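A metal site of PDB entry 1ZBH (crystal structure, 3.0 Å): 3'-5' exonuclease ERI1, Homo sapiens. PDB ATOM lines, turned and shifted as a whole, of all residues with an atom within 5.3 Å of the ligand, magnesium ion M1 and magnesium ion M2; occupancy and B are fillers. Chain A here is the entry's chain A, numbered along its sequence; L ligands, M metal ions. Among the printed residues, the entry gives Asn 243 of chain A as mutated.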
ATOM      1  N   ASP A  84      -4.977  17.022   9.163  1.00  0.00           N
ATOM      2  CA  ASP A  84      -4.241  16.310  10.211  1.00  0.00           C
ATOM      3  C   ASP A  84      -3.402  17.245  11.062  1.00  0.00           C
ATOM      4  O   ASP A  84      -2.248  17.547  10.742  1.00  0.00           O
ATOM      5  CB  ASP A  84      -3.379  15.183   9.630  1.00  0.00           C
ATOM      6  CG  ASP A  84      -2.854  14.263  10.714  1.00  0.00           C
ATOM      7  OD1 ASP A  84      -3.656  13.842  11.585  1.00  0.00           O
ATOM      8  OD2 ASP A  84      -1.644  13.950  10.705  1.00  0.00           O
ATOM      9  N   PHE A  85      -3.981  17.687  12.172  1.00  0.00           N
ATOM     10  CA  PHE A  85      -3.323  18.626  13.078  1.00  0.00           C
ATOM     11  C   PHE A  85      -2.058  18.031  13.664  1.00  0.00           C
ATOM     12  O   PHE A  85      -1.972  16.821  13.924  1.00  0.00           O
ATOM     13  CB  PHE A  85      -4.243  19.019  14.236  1.00  0.00           C
ATOM     14  CG  PHE A  85      -5.512  19.697  13.803  1.00  0.00           C
ATOM     15  CD1 PHE A  85      -5.466  20.887  13.084  1.00  0.00           C
ATOM     16  CD2 PHE A  85      -6.737  19.157  14.139  1.00  0.00           C
ATOM     17  CE1 PHE A  85      -6.634  21.525  12.683  1.00  0.00           C
ATOM     18  CE2 PHE A  85      -7.922  19.787  13.750  1.00  0.00           C
ATOM     19  CZ  PHE A  85      -7.868  20.967  13.026  1.00  0.00           C
ATOM     20  N   GLU A  86      -1.073  18.897  13.855  1.00  0.00           N
ATOM     21  CA  GLU A  86       0.018  18.636  14.761  1.00  0.00           C
ATOM     22  C   GLU A  86      -0.152  19.594  15.917  1.00  0.00           C
ATOM     23  O   GLU A  86      -0.617  20.718  15.727  1.00  0.00           O
ATOM     24  CB  GLU A  86       1.377  18.830  14.087  1.00  0.00           C
ATOM     25  CG  GLU A  86       1.655  17.867  12.928  1.00  0.00           C
ATOM     26  CD  GLU A  86       1.530  16.399  13.304  1.00  0.00           C
ATOM     27  OE1 GLU A  86       2.232  15.936  14.237  1.00  0.00           O
ATOM     28  OE2 GLU A  86       0.739  15.681  12.640  1.00  0.00           O
ATOM     29  N   ALA A  87       0.209  19.141  17.114  1.00  0.00           N
ATOM     30  CA  ALA A  87       0.042  19.944  18.323  1.00  0.00           C
ATOM     31  C   ALA A  87       1.246  19.773  19.250  1.00  0.00           C
ATOM     32  O   ALA A  87       1.968  18.789  19.145  1.00  0.00           O
ATOM     33  CB  ALA A  87      -1.242  19.552  19.040  1.00  0.00           C
ATOM     34  N   THR A  88       1.433  20.750  20.140  1.00  0.00           N
ATOM     35  CA  THR A  88       2.485  20.699  21.160  1.00  0.00           C
ATOM     36  C   THR A  88       2.372  19.438  22.008  1.00  0.00           C
ATOM     37  O   THR A  88       1.267  18.991  22.322  1.00  0.00           O
ATOM     38  CB  THR A  88       2.454  21.932  22.089  1.00  0.00           C
ATOM     39  OG1 THR A  88       1.170  22.024  22.728  1.00  0.00           O
ATOM     40  CG2 THR A  88       2.725  23.208  21.325  1.00  0.00           C
ATOM     41  N   CYS A  89       3.511  18.857  22.375  1.00  0.00           N
ATOM     42  CA  CYS A  89       3.555  17.646  23.192  1.00  0.00           C
ATOM     43  C   CYS A  89       4.892  17.499  23.900  1.00  0.00           C
ATOM     44  O   CYS A  89       5.889  18.086  23.474  1.00  0.00           O
ATOM     45  CB  CYS A  89       3.305  16.421  22.314  1.00  0.00           C
ATOM     46  SG  CYS A  89       4.490  16.224  20.970  1.00  0.00           S
ATOM     47  N   GLU A  90       4.909  16.721  24.983  1.00  0.00           N
ATOM     48  CA  GLU A  90       6.137  16.375  25.678  1.00  0.00           C
ATOM     49  C   GLU A  90       6.440  14.883  25.582  1.00  0.00           C
ATOM     50  O   GLU A  90       5.541  14.078  25.274  1.00  0.00           O
ATOM     51  CB  GLU A  90       6.074  16.786  27.152  1.00  0.00           C
ATOM     52  CG  GLU A  90       6.936  17.993  27.503  1.00  0.00           C
ATOM     53  CD  GLU A  90       6.203  19.303  27.333  1.00  0.00           C
ATOM     54  OE1 GLU A  90       5.824  19.642  26.185  1.00  0.00           O
ATOM     55  OE2 GLU A  90       5.997  20.009  28.346  1.00  0.00           O
ATOM     56  N   GLY A  92       6.804  11.157  26.356  1.00  0.00           N
ATOM     57  CA  GLY A  92       6.044  10.234  27.193  1.00  0.00           C
ATOM     58  C   GLY A  92       4.581  10.602  27.374  1.00  0.00           C
ATOM     59  O   GLY A  92       3.882   9.975  28.171  1.00  0.00           O
ATOM     60  N   ASN A  93       4.127  11.607  26.623  1.00  0.00           N
ATOM     61  CA  ASN A  93       2.735  12.046  26.611  1.00  0.00           C
ATOM     62  C   ASN A  93       2.135  12.258  28.019  1.00  0.00           C
ATOM     63  O   ASN A  93       1.265  11.483  28.437  1.00  0.00           O
ATOM     64  CB  ASN A  93       1.885  11.038  25.812  1.00  0.00           C
ATOM     65  CG  ASN A  93       0.659  11.665  25.169  1.00  0.00           C
ATOM     66  OD1 ASN A  93       0.763  12.648  24.433  1.00  0.00           O
ATOM     67  ND2 ASN A  93      -0.501  11.069  25.416  1.00  0.00           N
ATOM     68  N   HIS A  99      -2.636  20.839  25.352  1.00  0.00           N
ATOM     69  CA  HIS A  99      -2.263  20.757  23.942  1.00  0.00           C
ATOM     70  C   HIS A  99      -2.673  22.010  23.170  1.00  0.00           C
ATOM     71  O   HIS A  99      -3.726  22.596  23.442  1.00  0.00           O
ATOM     72  CB  HIS A  99      -2.900  19.531  23.300  1.00  0.00           C
ATOM     73  CG  HIS A  99      -2.293  18.232  23.729  1.00  0.00           C
ATOM     74  ND1 HIS A  99      -0.999  17.872  23.409  1.00  0.00           N
ATOM     75  CD2 HIS A  99      -2.797  17.201  24.446  1.00  0.00           C
ATOM     76  CE1 HIS A  99      -0.741  16.679  23.913  1.00  0.00           C
ATOM     77  NE2 HIS A  99      -1.817  16.256  24.548  1.00  0.00           N
ATOM     78  N   PHE A 135      11.299  17.066  22.459  1.00  0.00           N
ATOM     79  CA  PHE A 135      10.637  15.885  21.915  1.00  0.00           C
ATOM     80  C   PHE A 135       9.681  16.271  20.790  1.00  0.00           C
ATOM     81  O   PHE A 135       9.658  15.628  19.734  1.00  0.00           O
ATOM     82  CB  PHE A 135       9.874  15.143  23.029  1.00  0.00           C
ATOM     83  CG  PHE A 135       8.981  14.039  22.541  1.00  0.00           C
ATOM     84  CD1 PHE A 135       9.488  12.770  22.288  1.00  0.00           C
ATOM     85  CD2 PHE A 135       7.618  14.260  22.348  1.00  0.00           C
ATOM     86  CE1 PHE A 135       8.652  11.742  21.850  1.00  0.00           C
ATOM     87  CE2 PHE A 135       6.775  13.242  21.915  1.00  0.00           C
ATOM     88  CZ  PHE A 135       7.303  11.972  21.659  1.00  0.00           C
ATOM     89  N   LEU A 139       9.715  15.083  16.951  1.00  0.00           N
ATOM     90  CA  LEU A 139       8.646  14.280  16.395  1.00  0.00           C
ATOM     91  C   LEU A 139       8.053  14.917  15.145  1.00  0.00           C
ATOM     92  O   LEU A 139       8.161  14.364  14.048  1.00  0.00           O
ATOM     93  CB  LEU A 139       7.544  14.037  17.434  1.00  0.00           C
ATOM     94  CG  LEU A 139       6.354  13.158  17.021  1.00  0.00           C
ATOM     95  CD1 LEU A 139       6.725  11.680  17.109  1.00  0.00           C
ATOM     96  CD2 LEU A 139       5.143  13.469  17.879  1.00  0.00           C
ATOM     97  N   THR A 140       7.451  16.087  15.316  1.00  0.00           N
ATOM     98  CA  THR A 140       6.732  16.797  14.257  1.00  0.00           C
ATOM     99  C   THR A 140       7.626  17.344  13.158  1.00  0.00           C
ATOM    100  O   THR A 140       7.195  17.493  12.008  1.00  0.00           O
ATOM    101  CB  THR A 140       5.925  17.980  14.818  1.00  0.00           C
ATOM    102  OG1 THR A 140       6.809  18.877  15.494  1.00  0.00           O
ATOM    103  CG2 THR A 140       4.853  17.503  15.788  1.00  0.00           C
ATOM    104  N   ASP A 180      -7.198  10.915  10.370  1.00  0.00           N
ATOM    105  CA  ASP A 180      -6.680   9.653  10.895  1.00  0.00           C
ATOM    106  C   ASP A 180      -6.885   9.570  12.402  1.00  0.00           C
ATOM    107  O   ASP A 180      -6.139  10.176  13.184  1.00  0.00           O
ATOM    108  CB  ASP A 180      -5.192   9.474  10.552  1.00  0.00           C
ATOM    109  CG  ASP A 180      -4.603   8.187  11.129  1.00  0.00           C
ATOM    110  OD1 ASP A 180      -5.285   7.146  11.076  1.00  0.00           O
ATOM    111  OD2 ASP A 180      -3.465   8.232  11.635  1.00  0.00           O
ATOM    112  N   TRP A 183      -8.830  11.845  17.455  1.00  0.00           N
ATOM    113  CA  TRP A 183      -8.023  12.883  18.097  1.00  0.00           C
ATOM    114  C   TRP A 183      -8.171  14.288  17.479  1.00  0.00           C
ATOM    115  O   TRP A 183      -8.511  15.249  18.177  1.00  0.00           O
ATOM    116  CB  TRP A 183      -6.545  12.461  18.108  1.00  0.00           C
ATOM    117  CG  TRP A 183      -6.143  11.754  19.379  1.00  0.00           C
ATOM    118  CD1 TRP A 183      -6.971  11.267  20.350  1.00  0.00           C
ATOM    119  CD2 TRP A 183      -4.799  11.444  19.792  1.00  0.00           C
ATOM    120  NE1 TRP A 183      -6.233  10.681  21.357  1.00  0.00           N
ATOM    121  CE2 TRP A 183      -4.896  10.775  21.042  1.00  0.00           C
ATOM    122  CE3 TRP A 183      -3.528  11.670  19.250  1.00  0.00           C
ATOM    123  CZ2 TRP A 183      -3.772  10.333  21.748  1.00  0.00           C
ATOM    124  CZ3 TRP A 183      -2.401  11.226  19.942  1.00  0.00           C
ATOM    125  CH2 TRP A 183      -2.540  10.557  21.185  1.00  0.00           C
ATOM    126  N   ASP A 184      -7.944  14.389  16.176  1.00  0.00           N
ATOM    127  CA  ASP A 184      -7.895  15.685  15.493  1.00  0.00           C
ATOM    128  C   ASP A 184      -9.012  16.649  15.915  1.00  0.00           C
ATOM    129  O   ASP A 184      -8.747  17.740  16.417  1.00  0.00           O
ATOM    130  CB  ASP A 184      -7.858  15.481  13.977  1.00  0.00           C
ATOM    131  CG  ASP A 184      -6.484  15.033  13.487  1.00  0.00           C
ATOM    132  OD1 ASP A 184      -5.993  15.635  12.519  1.00  0.00           O
ATOM    133  OD2 ASP A 184      -5.898  14.089  14.063  1.00  0.00           O
ATOM    134  N   PHE A 188      -7.810  17.719  19.778  1.00  0.00           N
ATOM    135  CA  PHE A 188      -6.985  18.892  19.446  1.00  0.00           C
ATOM    136  C   PHE A 188      -7.769  20.157  19.157  1.00  0.00           C
ATOM    137  O   PHE A 188      -7.540  21.185  19.778  1.00  0.00           O
ATOM    138  CB  PHE A 188      -5.993  18.573  18.325  1.00  0.00           C
ATOM    139  CG  PHE A 188      -4.997  17.492  18.690  1.00  0.00           C
ATOM    140  CD1 PHE A 188      -4.235  17.596  19.861  1.00  0.00           C
ATOM    141  CD2 PHE A 188      -4.833  16.381  17.874  1.00  0.00           C
ATOM    142  CE1 PHE A 188      -3.335  16.598  20.210  1.00  0.00           C
ATOM    143  CE2 PHE A 188      -3.923  15.379  18.204  1.00  0.00           C
ATOM    144  CZ  PHE A 188      -3.177  15.485  19.387  1.00  0.00           C
ATOM    145  N   ARG A 211      -9.829   5.319  10.211  1.00  0.00           N
ATOM    146  CA  ARG A 211      -9.444   4.090  10.925  1.00  0.00           C
ATOM    147  C   ARG A 211     -10.630   3.156  11.129  1.00  0.00           C
ATOM    148  O   ARG A 211     -10.511   1.945  10.959  1.00  0.00           O
ATOM    149  CB  ARG A 211      -8.818   4.417  12.278  1.00  0.00           C
ATOM    150  CG  ARG A 211      -7.384   4.879  12.173  1.00  0.00           C
ATOM    151  CD  ARG A 211      -6.799   5.256  13.512  1.00  0.00           C
ATOM    152  NE  ARG A 211      -5.389   5.614  13.373  1.00  0.00           N
ATOM    153  CZ  ARG A 211      -4.719   6.420  14.200  1.00  0.00           C
ATOM    154  NH1 ARG A 211      -5.337   6.967  15.251  1.00  0.00           N
ATOM    155  NH2 ARG A 211      -3.446   6.680  13.972  1.00  0.00           N
ATOM    156  N   ASN A 243       5.054  12.168  10.538  1.00  0.00           N
ATOM    157  CA  ASN A 243       4.639  13.094  11.613  1.00  0.00           C
ATOM    158  C   ASN A 243       4.574  14.578  11.222  1.00  0.00           C
ATOM    159  O   ASN A 243       4.226  15.424  12.037  1.00  0.00           O
ATOM    160  CB  ASN A 243       5.462  12.878  12.900  1.00  0.00           C
ATOM    161  CG  ASN A 243       5.328  11.464  13.448  1.00  0.00           C
ATOM    162  OD1 ASN A 243       6.309  10.855  13.856  1.00  0.00           O
ATOM    163  ND2 ASN A 243       4.104  10.950  13.460  1.00  0.00           N
ATOM    164  N   CYS A 244       4.904  14.862   9.961  1.00  0.00           N
ATOM    165  CA  CYS A 244       4.715  16.197   9.405  1.00  0.00           C
ATOM    166  C   CYS A 244       3.269  16.286   8.904  1.00  0.00           C
ATOM    167  O   CYS A 244       2.888  15.593   7.960  1.00  0.00           O
ATOM    168  CB  CYS A 244       5.730  16.444   8.292  1.00  0.00           C
ATOM    169  SG  CYS A 244       5.255  17.593   6.986  1.00  0.00           S
ATOM    170  N   GLY A 245       2.474  17.129   9.568  1.00  0.00           N
ATOM    171  CA  GLY A 245       1.022  17.247   9.339  1.00  0.00           C
ATOM    172  C   GLY A 245       0.546  17.185   7.900  1.00  0.00           C
ATOM    173  O   GLY A 245      -0.320  16.376   7.569  1.00  0.00           O
ATOM    174  N   ASP A 248       1.485  13.854   6.330  1.00  0.00           N
ATOM    175  CA  ASP A 248       0.568  12.877   6.878  1.00  0.00           C
ATOM    176  C   ASP A 248      -0.746  12.935   6.116  1.00  0.00           C
ATOM    177  O   ASP A 248      -1.195  11.935   5.561  1.00  0.00           O
ATOM    178  CB  ASP A 248       0.320  13.126   8.365  1.00  0.00           C
ATOM    179  CG  ASP A 248       1.501  12.747   9.246  1.00  0.00           C
ATOM    180  OD1 ASP A 248       1.880  13.578  10.090  1.00  0.00           O
ATOM    181  OD2 ASP A 248       2.038  11.626   9.115  1.00  0.00           O
ATOM    182  N   ILE A 252      -2.647   9.981   4.113  1.00  0.00           N
ATOM    183  CA  ILE A 252      -4.025   9.633   4.473  1.00  0.00           C
ATOM    184  C   ILE A 252      -4.915   9.738   3.234  1.00  0.00           C
ATOM    185  O   ILE A 252      -5.781   8.884   3.019  1.00  0.00           O
ATOM    186  CB  ILE A 252      -4.561  10.524   5.625  1.00  0.00           C
ATOM    187  CG1 ILE A 252      -3.663  10.419   6.859  1.00  0.00           C
ATOM    188  CG2 ILE A 252      -5.985  10.129   5.999  1.00  0.00           C
ATOM    189  CD1 ILE A 252      -3.794  11.589   7.816  1.00  0.00           C
HETATM  190  P1  LIG L   1      -0.643  12.511  14.352  1.00  0.00           P
HETATM  191  O1  LIG L   1      -1.736  13.297  13.659  1.00  0.00           O
HETATM  192  O2  LIG L   1       0.739  12.694  13.749  1.00  0.00           O
HETATM  193  O3  LIG L   1      -1.015  11.095  14.662  1.00  0.00           O
HETATM  194  O4  LIG L   1      -0.511  13.195  15.805  1.00  0.00           O
HETATM  195  C1  LIG L   1      -0.277  14.594  15.901  1.00  0.00           C
HETATM  196  C2  LIG L   1      -0.094  15.050  17.331  1.00  0.00           C
HETATM  197  O5  LIG L   1      -0.332  14.013  18.292  1.00  0.00           O
HETATM  198  C3  LIG L   1       1.322  15.531  17.568  1.00  0.00           C
HETATM  199  O6  LIG L   1       1.460  16.920  17.278  1.00  0.00           O
HETATM  200  C4  LIG L   1       1.552  15.253  19.035  1.00  0.00           C
HETATM  201  O7  LIG L   1       1.191  16.390  19.827  1.00  0.00           O
HETATM  202  C5  LIG L   1       0.637  14.081  19.345  1.00  0.00           C
HETATM  203  N1  LIG L   1       1.459  12.850  19.381  1.00  0.00           N
HETATM  204  C6  LIG L   1       1.560  11.947  18.379  1.00  0.00           C
HETATM  205  N2  LIG L   1       2.388  10.930  18.719  1.00  0.00           N
HETATM  206  C7  LIG L   1       2.839  11.177  19.959  1.00  0.00           C
HETATM  207  C8  LIG L   1       3.744  10.495  20.908  1.00  0.00           C
HETATM  208  N3  LIG L   1       4.339   9.332  20.568  1.00  0.00           N
HETATM  209  N4  LIG L   1       3.953  11.082  22.121  1.00  0.00           N
HETATM  210  C9  LIG L   1       3.357  12.245  22.461  1.00  0.00           C
HETATM  211  N5  LIG L   1       2.524  12.921  21.634  1.00  0.00           N
HETATM  212  C10 LIG L   1       2.227  12.446  20.396  1.00  0.00           C
HETATM  213 MG    MG M   1       0.096  13.813  11.816  1.00  0.00          MG
HETATM  214 MG    MG M   2      -2.978  12.219  12.960  1.00  0.00          MG
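O1 of the ligand binds magnesium ion M2 (1.8 Å).
OD1 of Asp 84 is bound to magnesium ion M2 (2.2 Å).
Magnesium ion M2 has two donor atoms within binding distance.
Slightly farther from magnesium ion M2 lies an oxygen (O3) of the ligand (2.8 Å).
The backbone carbonyl oxygen (O) of Thr 88 is in hydrogen-bond range of a ring nitrogen (ND1) of His 99.
The side-chain carboxylate of Asp 180 is in salt-bridge range of the guanidinium group of Arg 211.
N of Asn 243 is in hydrogen-bond range of OD2 of Asp 248, at 3.4 Å.
The backbone NH of Phe 85 is in hydrogen-bond range of the side-chain carboxylate of Asp 184 (2.9 Å).
N of Cys 244 lies close to OD1 of Asp 248.
N of Phe 188 sits at hydrogen-bond distance from O of Trp 183 (3.0 Å).
The side-chain carboxylate (OD2) of Asp 84 is bound to magnesium ion M1, at 2.1 Å.
Magnesium ion M1 is bound by OE2 of Glu 86, 2.1 Å away.
Magnesium ion M1 is bound by O2 of the ligand, 2.3 Å away.
Magnesium ion M1 is bound by the side-chain carboxylate (OD1) of Asp 248 (2.5 Å).
Magnesium ion M1 has four donor atoms within binding distance.
Slightly farther from magnesium ion M1 lies an oxygen (O1) of the ligand (2.6 Å).
Asp 180 touches magnesium ion M2 (O to MG, 3.8 Å).
Asp 184 touches magnesium ion M2.
Phe 85 touches the ligand (O to C1, 3.4 Å).
Thr 88 touches the ligand (O to O7, 3.6 Å).
CZ of Phe 135 touches N4 of the ligand, at 3.5 Å.
CD2 of Leu 139 touches N2 of the ligand, at 3.8 Å.
Thr 140 touches the ligand (CG2 to O6, 3.8 Å).
Trp 183 touches the ligand.
Phe 188 touches the ligand (CZ to O5, 3.4 Å).
Asn 243 touches the ligand (ND2 to O2, 3.8 Å).
Of the 23 residues printed, 14 come within 4 Å of the ligand.
Along chain A the residues within 4 Å of the ligand span positions 84 to 248.
The nearest printed residue that does not touch the ligand is Glu 90 (4.01 Å).
An oxygen (O7) of the ligand sits at hydrogen-bond distance from the backbone carbonyl oxygen (O) of Ala 87 (2.6 Å).
SG of Cys 89 sits close to O7 of the ligand.
A nitrogen (N5) of the ligand sits close to the side-chain amide oxygen (OD1) of Asn 93, at 3.3 Å.
An oxygen (O6) of the ligand sits at hydrogen-bond distance from the backbone NH (N) of Ala 87 (2.6 Å).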
